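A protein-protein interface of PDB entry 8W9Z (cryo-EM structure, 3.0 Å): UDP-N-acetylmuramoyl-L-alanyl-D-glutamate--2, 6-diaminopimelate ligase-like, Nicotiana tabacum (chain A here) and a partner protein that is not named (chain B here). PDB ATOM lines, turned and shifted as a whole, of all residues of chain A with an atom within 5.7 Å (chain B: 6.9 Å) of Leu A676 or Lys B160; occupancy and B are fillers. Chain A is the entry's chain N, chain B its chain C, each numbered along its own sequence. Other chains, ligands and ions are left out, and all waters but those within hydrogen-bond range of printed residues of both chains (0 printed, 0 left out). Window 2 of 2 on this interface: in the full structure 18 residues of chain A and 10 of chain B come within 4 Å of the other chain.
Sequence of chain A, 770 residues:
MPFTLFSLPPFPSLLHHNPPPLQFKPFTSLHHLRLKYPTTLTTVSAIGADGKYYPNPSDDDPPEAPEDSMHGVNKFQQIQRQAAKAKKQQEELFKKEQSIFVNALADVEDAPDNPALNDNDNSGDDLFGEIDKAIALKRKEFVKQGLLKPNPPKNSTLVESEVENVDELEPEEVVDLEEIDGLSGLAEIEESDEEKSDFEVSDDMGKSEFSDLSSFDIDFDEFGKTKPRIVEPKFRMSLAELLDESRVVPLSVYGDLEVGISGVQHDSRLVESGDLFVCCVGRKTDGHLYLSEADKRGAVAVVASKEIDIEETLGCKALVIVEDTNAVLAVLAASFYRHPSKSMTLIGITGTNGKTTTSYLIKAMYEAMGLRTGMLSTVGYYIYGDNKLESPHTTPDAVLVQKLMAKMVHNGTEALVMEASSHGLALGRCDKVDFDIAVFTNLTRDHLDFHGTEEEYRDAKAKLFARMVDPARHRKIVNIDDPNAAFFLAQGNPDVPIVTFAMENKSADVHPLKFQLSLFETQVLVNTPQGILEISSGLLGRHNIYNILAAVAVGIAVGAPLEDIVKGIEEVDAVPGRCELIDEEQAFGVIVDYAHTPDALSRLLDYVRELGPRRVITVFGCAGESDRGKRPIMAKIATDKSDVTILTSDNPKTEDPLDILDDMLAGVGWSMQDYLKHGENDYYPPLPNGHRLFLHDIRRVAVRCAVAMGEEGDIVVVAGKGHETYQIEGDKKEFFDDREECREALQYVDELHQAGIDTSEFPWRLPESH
The side-chain hydroxyl of Thr B163 is in hydrogen-bond range of the guanidinium group of Arg B156, 3.3 Å away.
Among the printed residues, merely in contact across the chains: Leu A658 with Lys B160 (3.6 Å) and Leu A676 with Lys B160 (3.8 Å).
O of Gly A679 is in hydrogen-bond range of NH1 of Arg B156 (2.7 Å). NH2 of Arg B156 is in hydrogen-bond range of O of Glu A680 (2.8 Å).
Of the printed residues of chain B, Leu A658 touches Lys B160 (3.6 Å). Of the printed residues of chain B, Leu A676 touches Lys B160 (3.8 Å). Printed residues of chain B within 4 Å of Gly A679: Arg B156 (2.7 Å). Printed residues of chain A within 4 Å of Arg B156: Gly A679 and Glu A680. Of chain A, only Leu A658 (3.6 Å) and Leu A676 (3.8 Å) come within 4 Å of Lys B160. Asp B212 touches none of the printed residues of chain A. The nearest residue of chain A that does not touch Lys B160 is Met A672 (5.4 Å).
Of the 11 printed residues of chain B, 2 touch a printed residue of chain A. Printed residues of chain A that touch a printed residue of chain B: Leu A658, Leu A676, Gly A679 and Glu A680. Hydrophobic or aromatic side chains of chain A that line the printed part of chain B: Leu A658 and Leu A676. Along chain A the printed residues that touch a printed residue of chain B span positions 658 to 680. Among the printed residues, no Asp or Glu carboxylate lies within 4 Å of a Lys or Arg side-chain nitrogen of the other chain.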
ATOM      1  N   LEU A 658      13.947   4.462  16.824  1.00  0.00           N
ATOM      2  CA  LEU A 658      13.697   4.824  15.430  1.00  0.00           C
ATOM      3  C   LEU A 658      12.222   5.124  15.185  1.00  0.00           C
ATOM      4  O   LEU A 658      11.808   5.328  14.040  1.00  0.00           O
ATOM      5  CB  LEU A 658      14.180   3.724  14.478  1.00  0.00           C
ATOM      6  CG  LEU A 658      15.688   3.495  14.320  1.00  0.00           C
ATOM      7  CD1 LEU A 658      16.260   2.669  15.463  1.00  0.00           C
ATOM      8  CD2 LEU A 658      15.988   2.838  12.980  1.00  0.00           C
ATOM      9  N   SER A 671      10.949  12.225   6.448  1.00  0.00           N
ATOM     10  CA  SER A 671      10.681  10.893   6.963  1.00  0.00           C
ATOM     11  C   SER A 671      11.983  10.108   7.010  1.00  0.00           C
ATOM     12  O   SER A 671      12.909  10.368   6.235  1.00  0.00           O
ATOM     13  CB  SER A 671       9.650  10.154   6.103  1.00  0.00           C
ATOM     14  OG  SER A 671      10.114   9.993   4.775  1.00  0.00           O
ATOM     15  N   MET A 672      12.051   9.145   7.934  1.00  0.00           N
ATOM     16  CA  MET A 672      13.270   8.358   8.077  1.00  0.00           C
ATOM     17  C   MET A 672      13.601   7.593   6.804  1.00  0.00           C
ATOM     18  O   MET A 672      14.777   7.357   6.512  1.00  0.00           O
ATOM     19  CB  MET A 672      13.146   7.394   9.257  1.00  0.00           C
ATOM     20  CG  MET A 672      13.230   8.069  10.614  1.00  0.00           C
ATOM     21  SD  MET A 672      13.549   6.900  11.946  1.00  0.00           S
ATOM     22  CE  MET A 672      15.120   6.217  11.425  1.00  0.00           C
ATOM     23  N   GLN A 673      12.582   7.207   6.033  1.00  0.00           N
ATOM     24  CA  GLN A 673      12.832   6.516   4.773  1.00  0.00           C
ATOM     25  C   GLN A 673      13.587   7.408   3.796  1.00  0.00           C
ATOM     26  O   GLN A 673      14.512   6.952   3.114  1.00  0.00           O
ATOM     27  CB  GLN A 673      11.511   6.049   4.164  1.00  0.00           C
ATOM     28  CG  GLN A 673      10.650   5.244   5.118  1.00  0.00           C
ATOM     29  CD  GLN A 673       9.284   4.933   4.549  1.00  0.00           C
ATOM     30  OE1 GLN A 673       8.413   4.416   5.246  1.00  0.00           O
ATOM     31  NE2 GLN A 673       9.087   5.251   3.274  1.00  0.00           N
ATOM     32  N   ASP A 674      13.209   8.687   3.721  1.00  0.00           N
ATOM     33  CA  ASP A 674      13.886   9.603   2.810  1.00  0.00           C
ATOM     34  C   ASP A 674      15.335   9.822   3.223  1.00  0.00           C
ATOM     35  O   ASP A 674      16.238   9.802   2.378  1.00  0.00           O
ATOM     36  CB  ASP A 674      13.136  10.933   2.749  1.00  0.00           C
ATOM     37  CG  ASP A 674      11.723  10.782   2.222  1.00  0.00           C
ATOM     38  OD1 ASP A 674      11.326   9.642   1.899  1.00  0.00           O
ATOM     39  OD2 ASP A 674      11.008  11.802   2.130  1.00  0.00           O
ATOM     40  N   TYR A 675      15.583  10.019   4.520  1.00  0.00           N
ATOM     41  CA  TYR A 675      16.956  10.215   4.969  1.00  0.00           C
ATOM     42  C   TYR A 675      17.787   8.953   4.785  1.00  0.00           C
ATOM     43  O   TYR A 675      18.980   9.041   4.474  1.00  0.00           O
ATOM     44  CB  TYR A 675      16.983  10.661   6.429  1.00  0.00           C
ATOM     45  CG  TYR A 675      18.231  11.434   6.793  1.00  0.00           C
ATOM     46  CD1 TYR A 675      19.419  10.777   7.086  1.00  0.00           C
ATOM     47  CD2 TYR A 675      18.223  12.822   6.834  1.00  0.00           C
ATOM     48  CE1 TYR A 675      20.564  11.482   7.412  1.00  0.00           C
ATOM     49  CE2 TYR A 675      19.360  13.535   7.161  1.00  0.00           C
ATOM     50  CZ  TYR A 675      20.527  12.859   7.449  1.00  0.00           C
ATOM     51  OH  TYR A 675      21.663  13.563   7.775  1.00  0.00           O
ATOM     52  N   LEU A 676      17.182   7.776   4.957  1.00  0.00           N
ATOM     53  CA  LEU A 676      17.926   6.536   4.762  1.00  0.00           C
ATOM     54  C   LEU A 676      18.260   6.315   3.291  1.00  0.00           C
ATOM     55  O   LEU A 676      19.380   5.911   2.960  1.00  0.00           O
ATOM     56  CB  LEU A 676      17.139   5.353   5.322  1.00  0.00           C
ATOM     57  CG  LEU A 676      17.130   5.222   6.845  1.00  0.00           C
ATOM     58  CD1 LEU A 676      16.335   3.999   7.277  1.00  0.00           C
ATOM     59  CD2 LEU A 676      18.550   5.159   7.385  1.00  0.00           C
ATOM     60  N   LYS A 677      17.305   6.573   2.393  1.00  0.00           N
ATOM     61  CA  LYS A 677      17.589   6.429   0.970  1.00  0.00           C
ATOM     62  C   LYS A 677      18.535   7.508   0.462  1.00  0.00           C
ATOM     63  O   LYS A 677      19.199   7.301  -0.559  1.00  0.00           O
ATOM     64  CB  LYS A 677      16.289   6.437   0.159  1.00  0.00           C
ATOM     65  CG  LYS A 677      15.601   7.787   0.072  1.00  0.00           C
ATOM     66  CD  LYS A 677      14.306   7.696  -0.719  1.00  0.00           C
ATOM     67  CE  LYS A 677      14.555   7.191  -2.131  1.00  0.00           C
ATOM     68  NZ  LYS A 677      15.470   8.090  -2.888  1.00  0.00           N
ATOM     69  N   HIS A 678      18.613   8.652   1.149  1.00  0.00           N
ATOM     70  CA  HIS A 678      19.629   9.642   0.810  1.00  0.00           C
ATOM     71  C   HIS A 678      20.991   9.251   1.372  1.00  0.00           C
ATOM     72  O   HIS A 678      22.027   9.608   0.799  1.00  0.00           O
ATOM     73  CB  HIS A 678      19.216  11.021   1.323  1.00  0.00           C
ATOM     74  CG  HIS A 678      18.039  11.606   0.608  1.00  0.00           C
ATOM     75  ND1 HIS A 678      17.463  12.803   0.976  1.00  0.00           N
ATOM     76  CD2 HIS A 678      17.330  11.160  -0.456  1.00  0.00           C
ATOM     77  CE1 HIS A 678      16.449  13.068   0.170  1.00  0.00           C
ATOM     78  NE2 HIS A 678      16.347  12.086  -0.707  1.00  0.00           N
ATOM     79  N   GLY A 679      21.006   8.522   2.490  1.00  0.00           N
ATOM     80  CA  GLY A 679      22.253   8.074   3.081  1.00  0.00           C
ATOM     81  C   GLY A 679      23.014   7.076   2.235  1.00  0.00           C
ATOM     82  O   GLY A 679      24.239   6.980   2.365  1.00  0.00           O
ATOM     83  N   GLU A 680      22.316   6.328   1.378  1.00  0.00           N
ATOM     84  CA  GLU A 680      23.007   5.460   0.431  1.00  0.00           C
ATOM     85  C   GLU A 680      23.874   6.268  -0.524  1.00  0.00           C
ATOM     86  O   GLU A 680      24.897   5.772  -1.006  1.00  0.00           O
ATOM     87  CB  GLU A 680      21.995   4.619  -0.349  1.00  0.00           C
ATOM     88  N   ARG B 156      28.878  -1.086   4.073  1.00  0.00           N
ATOM     89  CA  ARG B 156      27.760  -1.120   5.007  1.00  0.00           C
ATOM     90  C   ARG B 156      26.780  -2.212   4.596  1.00  0.00           C
ATOM     91  O   ARG B 156      25.845  -1.954   3.827  1.00  0.00           O
ATOM     92  CB  ARG B 156      27.069   0.244   5.073  1.00  0.00           C
ATOM     93  CG  ARG B 156      27.004   0.982   3.744  1.00  0.00           C
ATOM     94  CD  ARG B 156      26.456   2.388   3.923  1.00  0.00           C
ATOM     95  NE  ARG B 156      26.502   3.154   2.680  1.00  0.00           N
ATOM     96  CZ  ARG B 156      26.132   4.426   2.573  1.00  0.00           C
ATOM     97  NH1 ARG B 156      25.689   5.082   3.636  1.00  0.00           N
ATOM     98  NH2 ARG B 156      26.208   5.043   1.402  1.00  0.00           N
ATOM     99  N   PRO B 157      26.968  -3.444   5.080  1.00  0.00           N
ATOM    100  CA  PRO B 157      26.078  -4.538   4.649  1.00  0.00           C
ATOM    101  C   PRO B 157      24.626  -4.327   5.035  1.00  0.00           C
ATOM    102  O   PRO B 157      23.735  -4.494   4.192  1.00  0.00           O
ATOM    103  CB  PRO B 157      26.678  -5.769   5.347  1.00  0.00           C
ATOM    104  CG  PRO B 157      28.086  -5.386   5.672  1.00  0.00           C
ATOM    105  CD  PRO B 157      28.047  -3.918   5.959  1.00  0.00           C
ATOM    106  N   ILE B 158      24.360  -3.964   6.286  1.00  0.00           N
ATOM    107  CA  ILE B 158      23.004  -3.733   6.766  1.00  0.00           C
ATOM    108  C   ILE B 158      22.713  -2.242   6.689  1.00  0.00           C
ATOM    109  O   ILE B 158      23.454  -1.427   7.250  1.00  0.00           O
ATOM    110  CB  ILE B 158      22.821  -4.258   8.200  1.00  0.00           C
ATOM    111  N   THR B 159      21.641  -1.885   5.986  1.00  0.00           N
ATOM    112  CA  THR B 159      21.223  -0.493   5.831  1.00  0.00           C
ATOM    113  C   THR B 159      19.826  -0.352   6.429  1.00  0.00           C
ATOM    114  O   THR B 159      18.819  -0.436   5.724  1.00  0.00           O
ATOM    115  CB  THR B 159      21.258  -0.074   4.357  1.00  0.00           C
ATOM    116  OG1 THR B 159      20.343  -0.883   3.608  1.00  0.00           O
ATOM    117  CG2 THR B 159      22.658  -0.251   3.791  1.00  0.00           C
ATOM    118  N   LYS B 160      19.777  -0.129   7.743  1.00  0.00           N
ATOM    119  CA  LYS B 160      18.525   0.118   8.442  1.00  0.00           C
ATOM    120  C   LYS B 160      18.635   1.222   9.485  1.00  0.00           C
ATOM    121  O   LYS B 160      17.601   1.695   9.966  1.00  0.00           O
ATOM    122  CB  LYS B 160      18.022  -1.166   9.123  1.00  0.00           C
ATOM    123  CG  LYS B 160      17.574  -2.249   8.158  1.00  0.00           C
ATOM    124  CD  LYS B 160      16.357  -1.807   7.365  1.00  0.00           C
ATOM    125  CE  LYS B 160      15.175  -1.540   8.278  1.00  0.00           C
ATOM    126  NZ  LYS B 160      14.803  -2.753   9.057  1.00  0.00           N
ATOM    127  N   LYS B 161      19.840   1.640   9.843  1.00  0.00           N
ATOM    128  CA  LYS B 161      20.091   2.673  10.834  1.00  0.00           C
ATOM    129  C   LYS B 161      20.999   3.726  10.222  1.00  0.00           C
ATOM    130  O   LYS B 161      21.786   3.428   9.317  1.00  0.00           O
ATOM    131  CB  LYS B 161      20.741   2.091  12.100  1.00  0.00           C
ATOM    132  CG  LYS B 161      19.781   1.378  13.047  1.00  0.00           C
ATOM    133  CD  LYS B 161      19.425  -0.020  12.562  1.00  0.00           C
ATOM    134  CE  LYS B 161      20.666  -0.882  12.391  1.00  0.00           C
ATOM    135  NZ  LYS B 161      20.330  -2.242  11.888  1.00  0.00           N
ATOM    136  N   PRO B 162      20.910   4.973  10.687  1.00  0.00           N
ATOM    137  CA  PRO B 162      21.745   6.031  10.105  1.00  0.00           C
ATOM    138  C   PRO B 162      23.224   5.763  10.344  1.00  0.00           C
ATOM    139  O   PRO B 162      23.654   5.490  11.467  1.00  0.00           O
ATOM    140  CB  PRO B 162      21.271   7.296  10.831  1.00  0.00           C
ATOM    141  CG  PRO B 162      20.637   6.800  12.090  1.00  0.00           C
ATOM    142  CD  PRO B 162      20.012   5.489  11.734  1.00  0.00           C
ATOM    143  N   THR B 163      24.003   5.845   9.268  1.00  0.00           N
ATOM    144  CA  THR B 163      25.433   5.575   9.300  1.00  0.00           C
ATOM    145  C   THR B 163      26.202   6.859   9.029  1.00  0.00           C
ATOM    146  O   THR B 163      25.756   7.710   8.254  1.00  0.00           O
ATOM    147  CB  THR B 163      25.821   4.508   8.268  1.00  0.00           C
ATOM    148  OG1 THR B 163      25.544   4.993   6.948  1.00  0.00           O
ATOM    149  CG2 THR B 163      25.034   3.229   8.507  1.00  0.00           C
ATOM    150  N   ARG B 197      27.281  -2.287  11.939  1.00  0.00           N
ATOM    151  CA  ARG B 197      26.473  -1.634  10.917  1.00  0.00           C
ATOM    152  C   ARG B 197      27.287  -1.340   9.662  1.00  0.00           C
ATOM    153  O   ARG B 197      26.754  -1.398   8.548  1.00  0.00           O
ATOM    154  CB  ARG B 197      25.861  -0.348  11.474  1.00  0.00           C
ATOM    155  CG  ARG B 197      24.938  -0.575  12.660  1.00  0.00           C
ATOM    156  CD  ARG B 197      24.356   0.730  13.175  1.00  0.00           C
ATOM    157  NE  ARG B 197      23.450   0.511  14.300  1.00  0.00           N
ATOM    158  CZ  ARG B 197      22.820   1.482  14.954  1.00  0.00           C
ATOM    159  NH1 ARG B 197      22.996   2.747  14.598  1.00  0.00           N
ATOM    160  NH2 ARG B 197      22.016   1.186  15.966  1.00  0.00           N
ATOM    161  N   ASP B 212      17.751  -7.670   5.610  1.00  0.00           N
ATOM    162  CA  ASP B 212      17.062  -6.410   5.327  1.00  0.00           C
ATOM    163  C   ASP B 212      17.146  -6.063   3.839  1.00  0.00           C
ATOM    164  O   ASP B 212      17.695  -5.041   3.430  1.00  0.00           O
ATOM    165  CB  ASP B 212      17.629  -5.292   6.195  1.00  0.00           C
ATOM    166  CG  ASP B 212      19.139  -5.170   6.086  1.00  0.00           C
ATOM    167  OD1 ASP B 212      19.739  -5.864   5.239  1.00  0.00           O
ATOM    168  OD2 ASP B 212      19.727  -4.377   6.850  1.00  0.00           O
ATOM    169  N   LEU B 213      16.579  -6.945   3.023  1.00  0.00           N
ATOM    170  CA  LEU B 213      16.531  -6.768   1.576  1.00  0.00           C
ATOM    171  C   LEU B 213      15.094  -6.452   1.179  1.00  0.00           C
ATOM    172  O   LEU B 213      14.204  -7.297   1.324  1.00  0.00           O
ATOM    173  CB  LEU B 213      17.044  -8.014   0.857  1.00  0.00           C
ATOM    174  CG  LEU B 213      17.188  -7.909  -0.663  1.00  0.00           C
ATOM    175  CD1 LEU B 213      18.140  -6.783  -1.035  1.00  0.00           C
ATOM    176  CD2 LEU B 213      17.662  -9.228  -1.249  1.00  0.00           C
